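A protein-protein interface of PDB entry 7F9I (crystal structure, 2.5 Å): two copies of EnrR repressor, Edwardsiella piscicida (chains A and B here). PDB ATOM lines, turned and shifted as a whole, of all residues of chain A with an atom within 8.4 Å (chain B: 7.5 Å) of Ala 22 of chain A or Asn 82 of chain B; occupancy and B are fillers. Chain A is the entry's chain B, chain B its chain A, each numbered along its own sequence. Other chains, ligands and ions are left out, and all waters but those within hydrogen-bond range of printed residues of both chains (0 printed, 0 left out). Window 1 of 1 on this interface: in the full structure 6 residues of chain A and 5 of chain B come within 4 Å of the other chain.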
ATOM      1  N   TRP A  19     -29.340 -34.506 -13.706  1.00  0.00           N
ATOM      2  CA  TRP A  19     -28.198 -33.606 -13.638  1.00  0.00           C
ATOM      3  C   TRP A  19     -28.376 -32.623 -12.490  1.00  0.00           C
ATOM      4  O   TRP A  19     -29.491 -32.186 -12.194  1.00  0.00           O
ATOM      5  CB  TRP A  19     -28.040 -32.830 -14.946  1.00  0.00           C
ATOM      6  CG  TRP A  19     -27.597 -33.637 -16.126  1.00  0.00           C
ATOM      7  CD1 TRP A  19     -27.860 -34.955 -16.374  1.00  0.00           C
ATOM      8  CD2 TRP A  19     -26.827 -33.166 -17.238  1.00  0.00           C
ATOM      9  NE1 TRP A  19     -27.290 -35.334 -17.567  1.00  0.00           N
ATOM     10  CE2 TRP A  19     -26.652 -34.253 -18.118  1.00  0.00           C
ATOM     11  CE3 TRP A  19     -26.265 -31.930 -17.571  1.00  0.00           C
ATOM     12  CZ2 TRP A  19     -25.939 -34.141 -19.310  1.00  0.00           C
ATOM     13  CZ3 TRP A  19     -25.560 -31.820 -18.755  1.00  0.00           C
ATOM     14  CH2 TRP A  19     -25.402 -32.920 -19.609  1.00  0.00           C
ATOM     15  N   HIS A  20     -27.270 -32.278 -11.838  1.00  0.00           N
ATOM     16  CA  HIS A  20     -27.298 -31.213 -10.852  1.00  0.00           C
ATOM     17  C   HIS A  20     -27.243 -29.846 -11.529  1.00  0.00           C
ATOM     18  O   HIS A  20     -26.852 -29.712 -12.693  1.00  0.00           O
ATOM     19  CB  HIS A  20     -26.139 -31.341  -9.870  1.00  0.00           C
ATOM     20  CG  HIS A  20     -26.314 -30.522  -8.630  1.00  0.00           C
ATOM     21  ND1 HIS A  20     -25.692 -29.306  -8.452  1.00  0.00           N
ATOM     22  CD2 HIS A  20     -27.042 -30.740  -7.510  1.00  0.00           C
ATOM     23  CE1 HIS A  20     -26.029 -28.809  -7.276  1.00  0.00           C
ATOM     24  NE2 HIS A  20     -26.846 -29.661  -6.683  1.00  0.00           N
ATOM     25  N   ARG A  21     -27.650 -28.825 -10.774  1.00  0.00           N
ATOM     26  CA  ARG A  21     -27.448 -27.427 -11.138  1.00  0.00           C
ATOM     27  C   ARG A  21     -26.026 -27.157 -11.615  1.00  0.00           C
ATOM     28  O   ARG A  21     -25.817 -26.427 -12.590  1.00  0.00           O
ATOM     29  CB  ARG A  21     -27.771 -26.533  -9.941  1.00  0.00           C
ATOM     30  CG  ARG A  21     -27.399 -25.078 -10.125  1.00  0.00           C
ATOM     31  CD  ARG A  21     -27.605 -24.313  -8.834  1.00  0.00           C
ATOM     32  NE  ARG A  21     -28.989 -23.895  -8.664  1.00  0.00           N
ATOM     33  CZ  ARG A  21     -29.532 -22.849  -9.270  1.00  0.00           C
ATOM     34  NH1 ARG A  21     -28.860 -22.149 -10.168  1.00  0.00           N
ATOM     35  NH2 ARG A  21     -30.786 -22.514  -8.986  1.00  0.00           N
ATOM     36  N   ALA A  22     -25.037 -27.745 -10.938  1.00  0.00           N
ATOM     37  CA  ALA A  22     -23.651 -27.508 -11.320  1.00  0.00           C
ATOM     38  C   ALA A  22     -23.309 -28.197 -12.632  1.00  0.00           C
ATOM     39  O   ALA A  22     -22.485 -27.688 -13.399  1.00  0.00           O
ATOM     40  CB  ALA A  22     -22.713 -27.977 -10.209  1.00  0.00           C
ATOM     41  N   ASP A  23     -23.932 -29.345 -12.910  1.00  0.00           N
ATOM     42  CA  ASP A  23     -23.727 -30.012 -14.193  1.00  0.00           C
ATOM     43  C   ASP A  23     -24.345 -29.210 -15.329  1.00  0.00           C
ATOM     44  O   ASP A  23     -23.732 -29.035 -16.389  1.00  0.00           O
ATOM     45  CB  ASP A  23     -24.320 -31.418 -14.151  1.00  0.00           C
ATOM     46  CG  ASP A  23     -23.922 -32.177 -12.912  1.00  0.00           C
ATOM     47  OD1 ASP A  23     -22.833 -31.896 -12.366  1.00  0.00           O
ATOM     48  OD2 ASP A  23     -24.702 -33.053 -12.482  1.00  0.00           O
ATOM     49  N   ILE A  24     -25.572 -28.731 -15.130  1.00  0.00           N
ATOM     50  CA  ILE A  24     -26.267 -27.987 -16.175  1.00  0.00           C
ATOM     51  C   ILE A  24     -25.540 -26.682 -16.468  1.00  0.00           C
ATOM     52  O   ILE A  24     -25.245 -26.359 -17.625  1.00  0.00           O
ATOM     53  CB  ILE A  24     -27.730 -27.744 -15.767  1.00  0.00           C
ATOM     54  CG1 ILE A  24     -28.463 -29.080 -15.634  1.00  0.00           C
ATOM     55  CG2 ILE A  24     -28.424 -26.852 -16.787  1.00  0.00           C
ATOM     56  CD1 ILE A  24     -29.766 -28.997 -14.892  1.00  0.00           C
ATOM     57  N   VAL A  25     -25.245 -25.910 -15.416  1.00  0.00           N
ATOM     58  CA  VAL A  25     -24.531 -24.641 -15.566  1.00  0.00           C
ATOM     59  C   VAL A  25     -23.222 -24.849 -16.319  1.00  0.00           C
ATOM     60  O   VAL A  25     -22.951 -24.190 -17.330  1.00  0.00           O
ATOM     61  CB  VAL A  25     -24.289 -23.995 -14.191  1.00  0.00           C
ATOM     62  CG1 VAL A  25     -23.202 -22.936 -14.281  1.00  0.00           C
ATOM     63  CG2 VAL A  25     -25.579 -23.389 -13.657  1.00  0.00           C
ATOM     64  N   ALA A  26     -22.384 -25.760 -15.819  1.00  0.00           N
ATOM     65  CA  ALA A  26     -21.099 -26.041 -16.456  1.00  0.00           C
ATOM     66  C   ALA A  26     -21.258 -26.323 -17.946  1.00  0.00           C
ATOM     67  O   ALA A  26     -20.509 -25.791 -18.774  1.00  0.00           O
ATOM     68  CB  ALA A  26     -20.411 -27.214 -15.757  1.00  0.00           C
ATOM     69  N   ALA A  27     -22.229 -27.167 -18.305  1.00  0.00           N
ATOM     70  CA  ALA A  27     -22.414 -27.537 -19.707  1.00  0.00           C
ATOM     71  C   ALA A  27     -22.785 -26.329 -20.560  1.00  0.00           C
ATOM     72  O   ALA A  27     -22.320 -26.195 -21.698  1.00  0.00           O
ATOM     73  CB  ALA A  27     -23.476 -28.628 -19.827  1.00  0.00           C
ATOM     74  N   LEU A  28     -23.643 -25.450 -20.037  1.00  0.00           N
ATOM     75  CA  LEU A  28     -23.942 -24.197 -20.722  1.00  0.00           C
ATOM     76  C   LEU A  28     -22.688 -23.345 -20.888  1.00  0.00           C
ATOM     77  O   LEU A  28     -22.408 -22.840 -21.982  1.00  0.00           O
ATOM     78  CB  LEU A  28     -25.030 -23.438 -19.964  1.00  0.00           C
ATOM     79  CG  LEU A  28     -26.416 -24.074 -20.081  1.00  0.00           C
ATOM     80  CD1 LEU A  28     -27.362 -23.458 -19.083  1.00  0.00           C
ATOM     81  CD2 LEU A  28     -26.966 -23.916 -21.496  1.00  0.00           C
ATOM     82  N   HIS A  29     -21.927 -23.159 -19.804  1.00  0.00           N
ATOM     83  CA  HIS A  29     -20.687 -22.391 -19.888  1.00  0.00           C
ATOM     84  C   HIS A  29     -19.718 -22.982 -20.904  1.00  0.00           C
ATOM     85  O   HIS A  29     -18.942 -22.244 -21.522  1.00  0.00           O
ATOM     86  CB  HIS A  29     -20.029 -22.302 -18.510  1.00  0.00           C
ATOM     87  CG  HIS A  29     -20.686 -21.316 -17.595  1.00  0.00           C
ATOM     88  ND1 HIS A  29     -22.053 -21.248 -17.435  1.00  0.00           N
ATOM     89  CD2 HIS A  29     -20.165 -20.353 -16.798  1.00  0.00           C
ATOM     90  CE1 HIS A  29     -22.347 -20.289 -16.577  1.00  0.00           C
ATOM     91  NE2 HIS A  29     -21.220 -19.729 -16.176  1.00  0.00           N
ATOM     92  N   MET A  53     -33.539 -25.646 -12.103  1.00  0.00           N
ATOM     93  CA  MET A  53     -32.394 -26.466 -11.721  1.00  0.00           C
ATOM     94  C   MET A  53     -32.729 -27.379 -10.551  1.00  0.00           C
ATOM     95  O   MET A  53     -32.175 -28.478 -10.448  1.00  0.00           O
ATOM     96  CB  MET A  53     -31.191 -25.587 -11.366  1.00  0.00           C
ATOM     97  CG  MET A  53     -30.853 -24.497 -12.371  1.00  0.00           C
ATOM     98  SD  MET A  53     -29.901 -25.074 -13.787  1.00  0.00           S
ATOM     99  CE  MET A  53     -31.205 -25.564 -14.914  1.00  0.00           C
ATOM    100  N   GLU A  54     -33.617 -26.939  -9.656  1.00  0.00           N
ATOM    101  CA  GLU A  54     -34.040 -27.739  -8.512  1.00  0.00           C
ATOM    102  C   GLU A  54     -35.379 -28.433  -8.729  1.00  0.00           C
ATOM    103  O   GLU A  54     -35.504 -29.628  -8.451  1.00  0.00           O
ATOM    104  CB  GLU A  54     -34.115 -26.867  -7.252  1.00  0.00           C
ATOM    105  CG  GLU A  54     -32.790 -26.675  -6.534  1.00  0.00           C
ATOM    106  CD  GLU A  54     -32.071 -25.416  -6.972  1.00  0.00           C
ATOM    107  OE1 GLU A  54     -30.922 -25.523  -7.450  1.00  0.00           O
ATOM    108  OE2 GLU A  54     -32.655 -24.320  -6.838  1.00  0.00           O
ATOM    109  N   ASP B  18     -12.567 -27.336 -13.588  1.00  0.00           N
ATOM    110  CA  ASP B  18     -12.654 -28.662 -12.991  1.00  0.00           C
ATOM    111  C   ASP B  18     -11.656 -29.609 -13.644  1.00  0.00           C
ATOM    112  O   ASP B  18     -11.268 -29.439 -14.803  1.00  0.00           O
ATOM    113  CB  ASP B  18     -14.061 -29.243 -13.135  1.00  0.00           C
ATOM    114  CG  ASP B  18     -15.049 -28.648 -12.147  1.00  0.00           C
ATOM    115  OD1 ASP B  18     -16.264 -28.860 -12.325  1.00  0.00           O
ATOM    116  OD2 ASP B  18     -14.626 -27.903 -11.240  1.00  0.00           O
ATOM    117  N   GLU B  54     -18.034 -37.244 -14.402  1.00  0.00           N
ATOM    118  CA  GLU B  54     -18.795 -36.317 -15.233  1.00  0.00           C
ATOM    119  C   GLU B  54     -19.767 -35.455 -14.435  1.00  0.00           C
ATOM    120  O   GLU B  54     -19.824 -34.239 -14.645  1.00  0.00           O
ATOM    121  CB  GLU B  54     -19.561 -37.077 -16.324  1.00  0.00           C
ATOM    122  CG  GLU B  54     -18.683 -37.837 -17.309  1.00  0.00           C
ATOM    123  CD  GLU B  54     -18.632 -39.323 -17.012  1.00  0.00           C
ATOM    124  OE1 GLU B  54     -17.568 -39.806 -16.569  1.00  0.00           O
ATOM    125  OE2 GLU B  54     -19.658 -40.007 -17.221  1.00  0.00           O
ATOM    126  N   ARG B  55     -20.542 -36.052 -13.533  1.00  0.00           N
ATOM    127  CA  ARG B  55     -21.667 -35.369 -12.907  1.00  0.00           C
ATOM    128  C   ARG B  55     -21.538 -35.375 -11.388  1.00  0.00           C
ATOM    129  O   ARG B  55     -21.273 -36.416 -10.775  1.00  0.00           O
ATOM    130  CB  ARG B  55     -22.993 -35.985 -13.359  1.00  0.00           C
ATOM    131  CG  ARG B  55     -23.552 -35.296 -14.608  1.00  0.00           C
ATOM    132  CD  ARG B  55     -24.806 -35.964 -15.160  1.00  0.00           C
ATOM    133  NE  ARG B  55     -24.860 -37.389 -14.862  1.00  0.00           N
ATOM    134  CZ  ARG B  55     -24.204 -38.322 -15.540  1.00  0.00           C
ATOM    135  NH1 ARG B  55     -23.429 -38.013 -16.568  1.00  0.00           N
ATOM    136  NH2 ARG B  55     -24.331 -39.596 -15.178  1.00  0.00           N
ATOM    137  N   HIS B  56     -21.732 -34.191 -10.806  1.00  0.00           N
ATOM    138  CA  HIS B  56     -21.513 -33.911  -9.390  1.00  0.00           C
ATOM    139  C   HIS B  56     -22.235 -34.888  -8.464  1.00  0.00           C
ATOM    140  O   HIS B  56     -23.438 -35.126  -8.603  1.00  0.00           O
ATOM    141  CB  HIS B  56     -21.973 -32.475  -9.121  1.00  0.00           C
ATOM    142  CG  HIS B  56     -22.101 -32.127  -7.673  1.00  0.00           C
ATOM    143  ND1 HIS B  56     -21.039 -32.171  -6.798  1.00  0.00           N
ATOM    144  CD2 HIS B  56     -23.164 -31.696  -6.955  1.00  0.00           C
ATOM    145  CE1 HIS B  56     -21.445 -31.794  -5.599  1.00  0.00           C
ATOM    146  NE2 HIS B  56     -22.731 -31.503  -5.666  1.00  0.00           N
ATOM    147  N   TRP B  76     -12.652 -30.054  -8.018  1.00  0.00           N
ATOM    148  CA  TRP B  76     -13.857 -29.531  -8.662  1.00  0.00           C
ATOM    149  C   TRP B  76     -14.165 -28.123  -8.167  1.00  0.00           C
ATOM    150  O   TRP B  76     -15.153 -27.909  -7.448  1.00  0.00           O
ATOM    151  CB  TRP B  76     -15.049 -30.452  -8.415  1.00  0.00           C
ATOM    152  CG  TRP B  76     -14.911 -31.803  -9.037  1.00  0.00           C
ATOM    153  CD1 TRP B  76     -15.147 -32.132 -10.341  1.00  0.00           C
ATOM    154  CD2 TRP B  76     -14.517 -33.015  -8.382  1.00  0.00           C
ATOM    155  NE1 TRP B  76     -14.923 -33.472 -10.539  1.00  0.00           N
ATOM    156  CE2 TRP B  76     -14.535 -34.037  -9.352  1.00  0.00           C
ATOM    157  CE3 TRP B  76     -14.150 -33.338  -7.071  1.00  0.00           C
ATOM    158  CZ2 TRP B  76     -14.200 -35.355  -9.055  1.00  0.00           C
ATOM    159  CZ3 TRP B  76     -13.814 -34.652  -6.779  1.00  0.00           C
ATOM    160  CH2 TRP B  76     -13.843 -35.642  -7.767  1.00  0.00           C
ATOM    161  N   PRO B  77     -13.346 -27.132  -8.529  1.00  0.00           N
ATOM    162  CA  PRO B  77     -13.655 -25.753  -8.118  1.00  0.00           C
ATOM    163  C   PRO B  77     -14.980 -25.236  -8.653  1.00  0.00           C
ATOM    164  O   PRO B  77     -15.660 -24.471  -7.959  1.00  0.00           O
ATOM    165  CB  PRO B  77     -12.465 -24.951  -8.666  1.00  0.00           C
ATOM    166  CG  PRO B  77     -11.933 -25.785  -9.781  1.00  0.00           C
ATOM    167  CD  PRO B  77     -12.117 -27.200  -9.338  1.00  0.00           C
ATOM    168  N   GLN B  78     -15.370 -25.622  -9.871  1.00  0.00           N
ATOM    169  CA  GLN B  78     -16.590 -25.074 -10.457  1.00  0.00           C
ATOM    170  C   GLN B  78     -17.835 -25.720  -9.864  1.00  0.00           C
ATOM    171  O   GLN B  78     -18.807 -25.026  -9.541  1.00  0.00           O
ATOM    172  CB  GLN B  78     -16.602 -25.261 -11.976  1.00  0.00           C
ATOM    173  CG  GLN B  78     -15.344 -24.859 -12.713  1.00  0.00           C
ATOM    174  CD  GLN B  78     -15.421 -25.228 -14.179  1.00  0.00           C
ATOM    175  OE1 GLN B  78     -14.537 -25.897 -14.717  1.00  0.00           O
ATOM    176  NE2 GLN B  78     -16.472 -24.759 -14.846  1.00  0.00           N
ATOM    177  N   ARG B  79     -17.839 -27.056  -9.770  1.00  0.00           N
ATOM    178  CA  ARG B  79     -18.944 -27.774  -9.137  1.00  0.00           C
ATOM    179  C   ARG B  79     -19.305 -27.171  -7.790  1.00  0.00           C
ATOM    180  O   ARG B  79     -20.487 -26.998  -7.470  1.00  0.00           O
ATOM    181  CB  ARG B  79     -18.589 -29.251  -8.963  1.00  0.00           C
ATOM    182  CG  ARG B  79     -18.879 -30.129 -10.163  1.00  0.00           C
ATOM    183  CD  ARG B  79     -18.538 -31.577  -9.853  1.00  0.00           C
ATOM    184  NE  ARG B  79     -18.388 -32.379 -11.062  1.00  0.00           N
ATOM    185  CZ  ARG B  79     -18.086 -33.669 -11.069  1.00  0.00           C
ATOM    186  NH1 ARG B  79     -17.918 -34.346  -9.946  1.00  0.00           N
ATOM    187  NH2 ARG B  79     -17.943 -34.295 -12.235  1.00  0.00           N
ATOM    188  N   TYR B  80     -18.297 -26.846  -6.983  1.00  0.00           N
ATOM    189  CA  TYR B  80     -18.538 -26.322  -5.649  1.00  0.00           C
ATOM    190  C   TYR B  80     -18.828 -24.829  -5.651  1.00  0.00           C
ATOM    191  O   TYR B  80     -19.383 -24.317  -4.674  1.00  0.00           O
ATOM    192  CB  TYR B  80     -17.347 -26.651  -4.745  1.00  0.00           C
ATOM    193  CG  TYR B  80     -17.327 -28.108  -4.347  1.00  0.00           C
ATOM    194  CD1 TYR B  80     -17.071 -29.102  -5.286  1.00  0.00           C
ATOM    195  CD2 TYR B  80     -17.595 -28.495  -3.041  1.00  0.00           C
ATOM    196  CE1 TYR B  80     -17.068 -30.436  -4.931  1.00  0.00           C
ATOM    197  CE2 TYR B  80     -17.593 -29.828  -2.678  1.00  0.00           C
ATOM    198  CZ  TYR B  80     -17.329 -30.794  -3.627  1.00  0.00           C
ATOM    199  OH  TYR B  80     -17.328 -32.121  -3.267  1.00  0.00           O
ATOM    200  N   ARG B  81     -18.462 -24.117  -6.715  1.00  0.00           N
ATOM    201  CA  ARG B  81     -18.916 -22.742  -6.869  1.00  0.00           C
ATOM    202  C   ARG B  81     -20.323 -22.654  -7.451  1.00  0.00           C
ATOM    203  O   ARG B  81     -21.071 -21.736  -7.100  1.00  0.00           O
ATOM    204  CB  ARG B  81     -17.941 -21.959  -7.747  1.00  0.00           C
ATOM    205  N   ASN B  82     -20.706 -23.586  -8.329  1.00  0.00           N
ATOM    206  CA  ASN B  82     -22.014 -23.544  -8.969  1.00  0.00           C
ATOM    207  C   ASN B  82     -23.110 -24.251  -8.167  1.00  0.00           C
ATOM    208  O   ASN B  82     -24.062 -24.765  -8.767  1.00  0.00           O
ATOM    209  CB  ASN B  82     -21.932 -24.176 -10.361  1.00  0.00           C
ATOM    210  CG  ASN B  82     -21.058 -23.391 -11.314  1.00  0.00           C
ATOM    211  OD1 ASN B  82     -20.885 -22.178 -11.176  1.00  0.00           O
ATOM    212  ND2 ASN B  82     -20.470 -24.094 -12.275  1.00  0.00           N
ATOM    213  N   LYS B  83     -23.028 -24.260  -6.842  1.00  0.00           N
ATOM    214  CA  LYS B  83     -24.144 -24.755  -6.041  1.00  0.00           C
ATOM    215  C   LYS B  83     -24.481 -23.773  -4.929  1.00  0.00           C
ATOM    216  O   LYS B  83     -25.038 -24.155  -3.901  1.00  0.00           O
ATOM    217  CB  LYS B  83     -23.833 -26.135  -5.461  1.00  0.00           C
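The backbone NH of His 56 of chain B is in hydrogen-bond range of the side-chain carboxylate of Asp 23 of chain A.
Among the printed residues, merely in contact across the chains: Trp 19 of chain A with Arg 55 of chain B, His 20 of chain A with His 56 of chain B, His 20 of chain A with Lys 83 of chain B, Arg 21 of chain A with Asn 82 of chain B, Ala 22 of chain A with Arg 79 of chain B, Ala 22 of chain A with Asn 82 of chain B, Asp 23 of chain A with Arg 55 of chain B and Val 25 of chain A with Asn 82 of chain B.
Ala 22 of chain A touches two residues of chain B.
Of the printed residues of chain B, Val 25 of chain A touches Asn 82 (3.6 Å).
Printed residues of chain A within 4 Å of Arg 55 of chain B: Trp 19 and Asp 23.
Of the printed residues of chain A, His 56 of chain B touches His 20 (3.8 Å) and Asp 23 (3.0 Å).
Tyr 80 of chain B touches none of the printed residues of chain A.
Printed residues of chain A within 4 Å of Lys 83 of chain B: His 20.
The backbone carbonyl oxygen (O) of Glu 54 of chain B sits at hydrogen-bond distance from the guanidinium group (NH2) of Arg 79 of chain B, at 3.1 Å.
O of Gln 78 of chain B lies close to ND2 of Asn 82 of chain B (3.3 Å).
N of Ala 22 of chain A is in hydrogen-bond range of ND1 of His 20 of chain A, at 3.0 Å.
The side-chain carboxylate of Asp 23 of chain A lies within hydrogen-bond range of the backbone NH of His 20 of chain A (2.8 Å).
The side-chain carboxylate of Glu 54 of chain A lies within salt-bridge range of the guanidinium group of Arg 21 of chain A (2.8 Å).
O of Val 25 of chain A lies within hydrogen-bond range of ND1 of His 29 of chain A.
1 position is printed for both chains.
Of the 9 pairs that touch across the chains among the printed residues, none has its exchanged pair printed and touching as well.
Printed residues of chain A that touch a printed residue of chain B: Trp 19, His 20, Arg 21, Ala 22, Asp 23 and Val 25.
Hydrophobic or aromatic side chains of chain A that line the printed part of chain B: Trp 19, His 20, Ala 22 and Val 25.
Hydrophobic or aromatic side chains of chain B that line the printed part of chain A: His 56.
Among the printed residues, no Asp or Glu carboxylate lies within 4 Å of a Lys or Arg side-chain nitrogen of the other chain.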
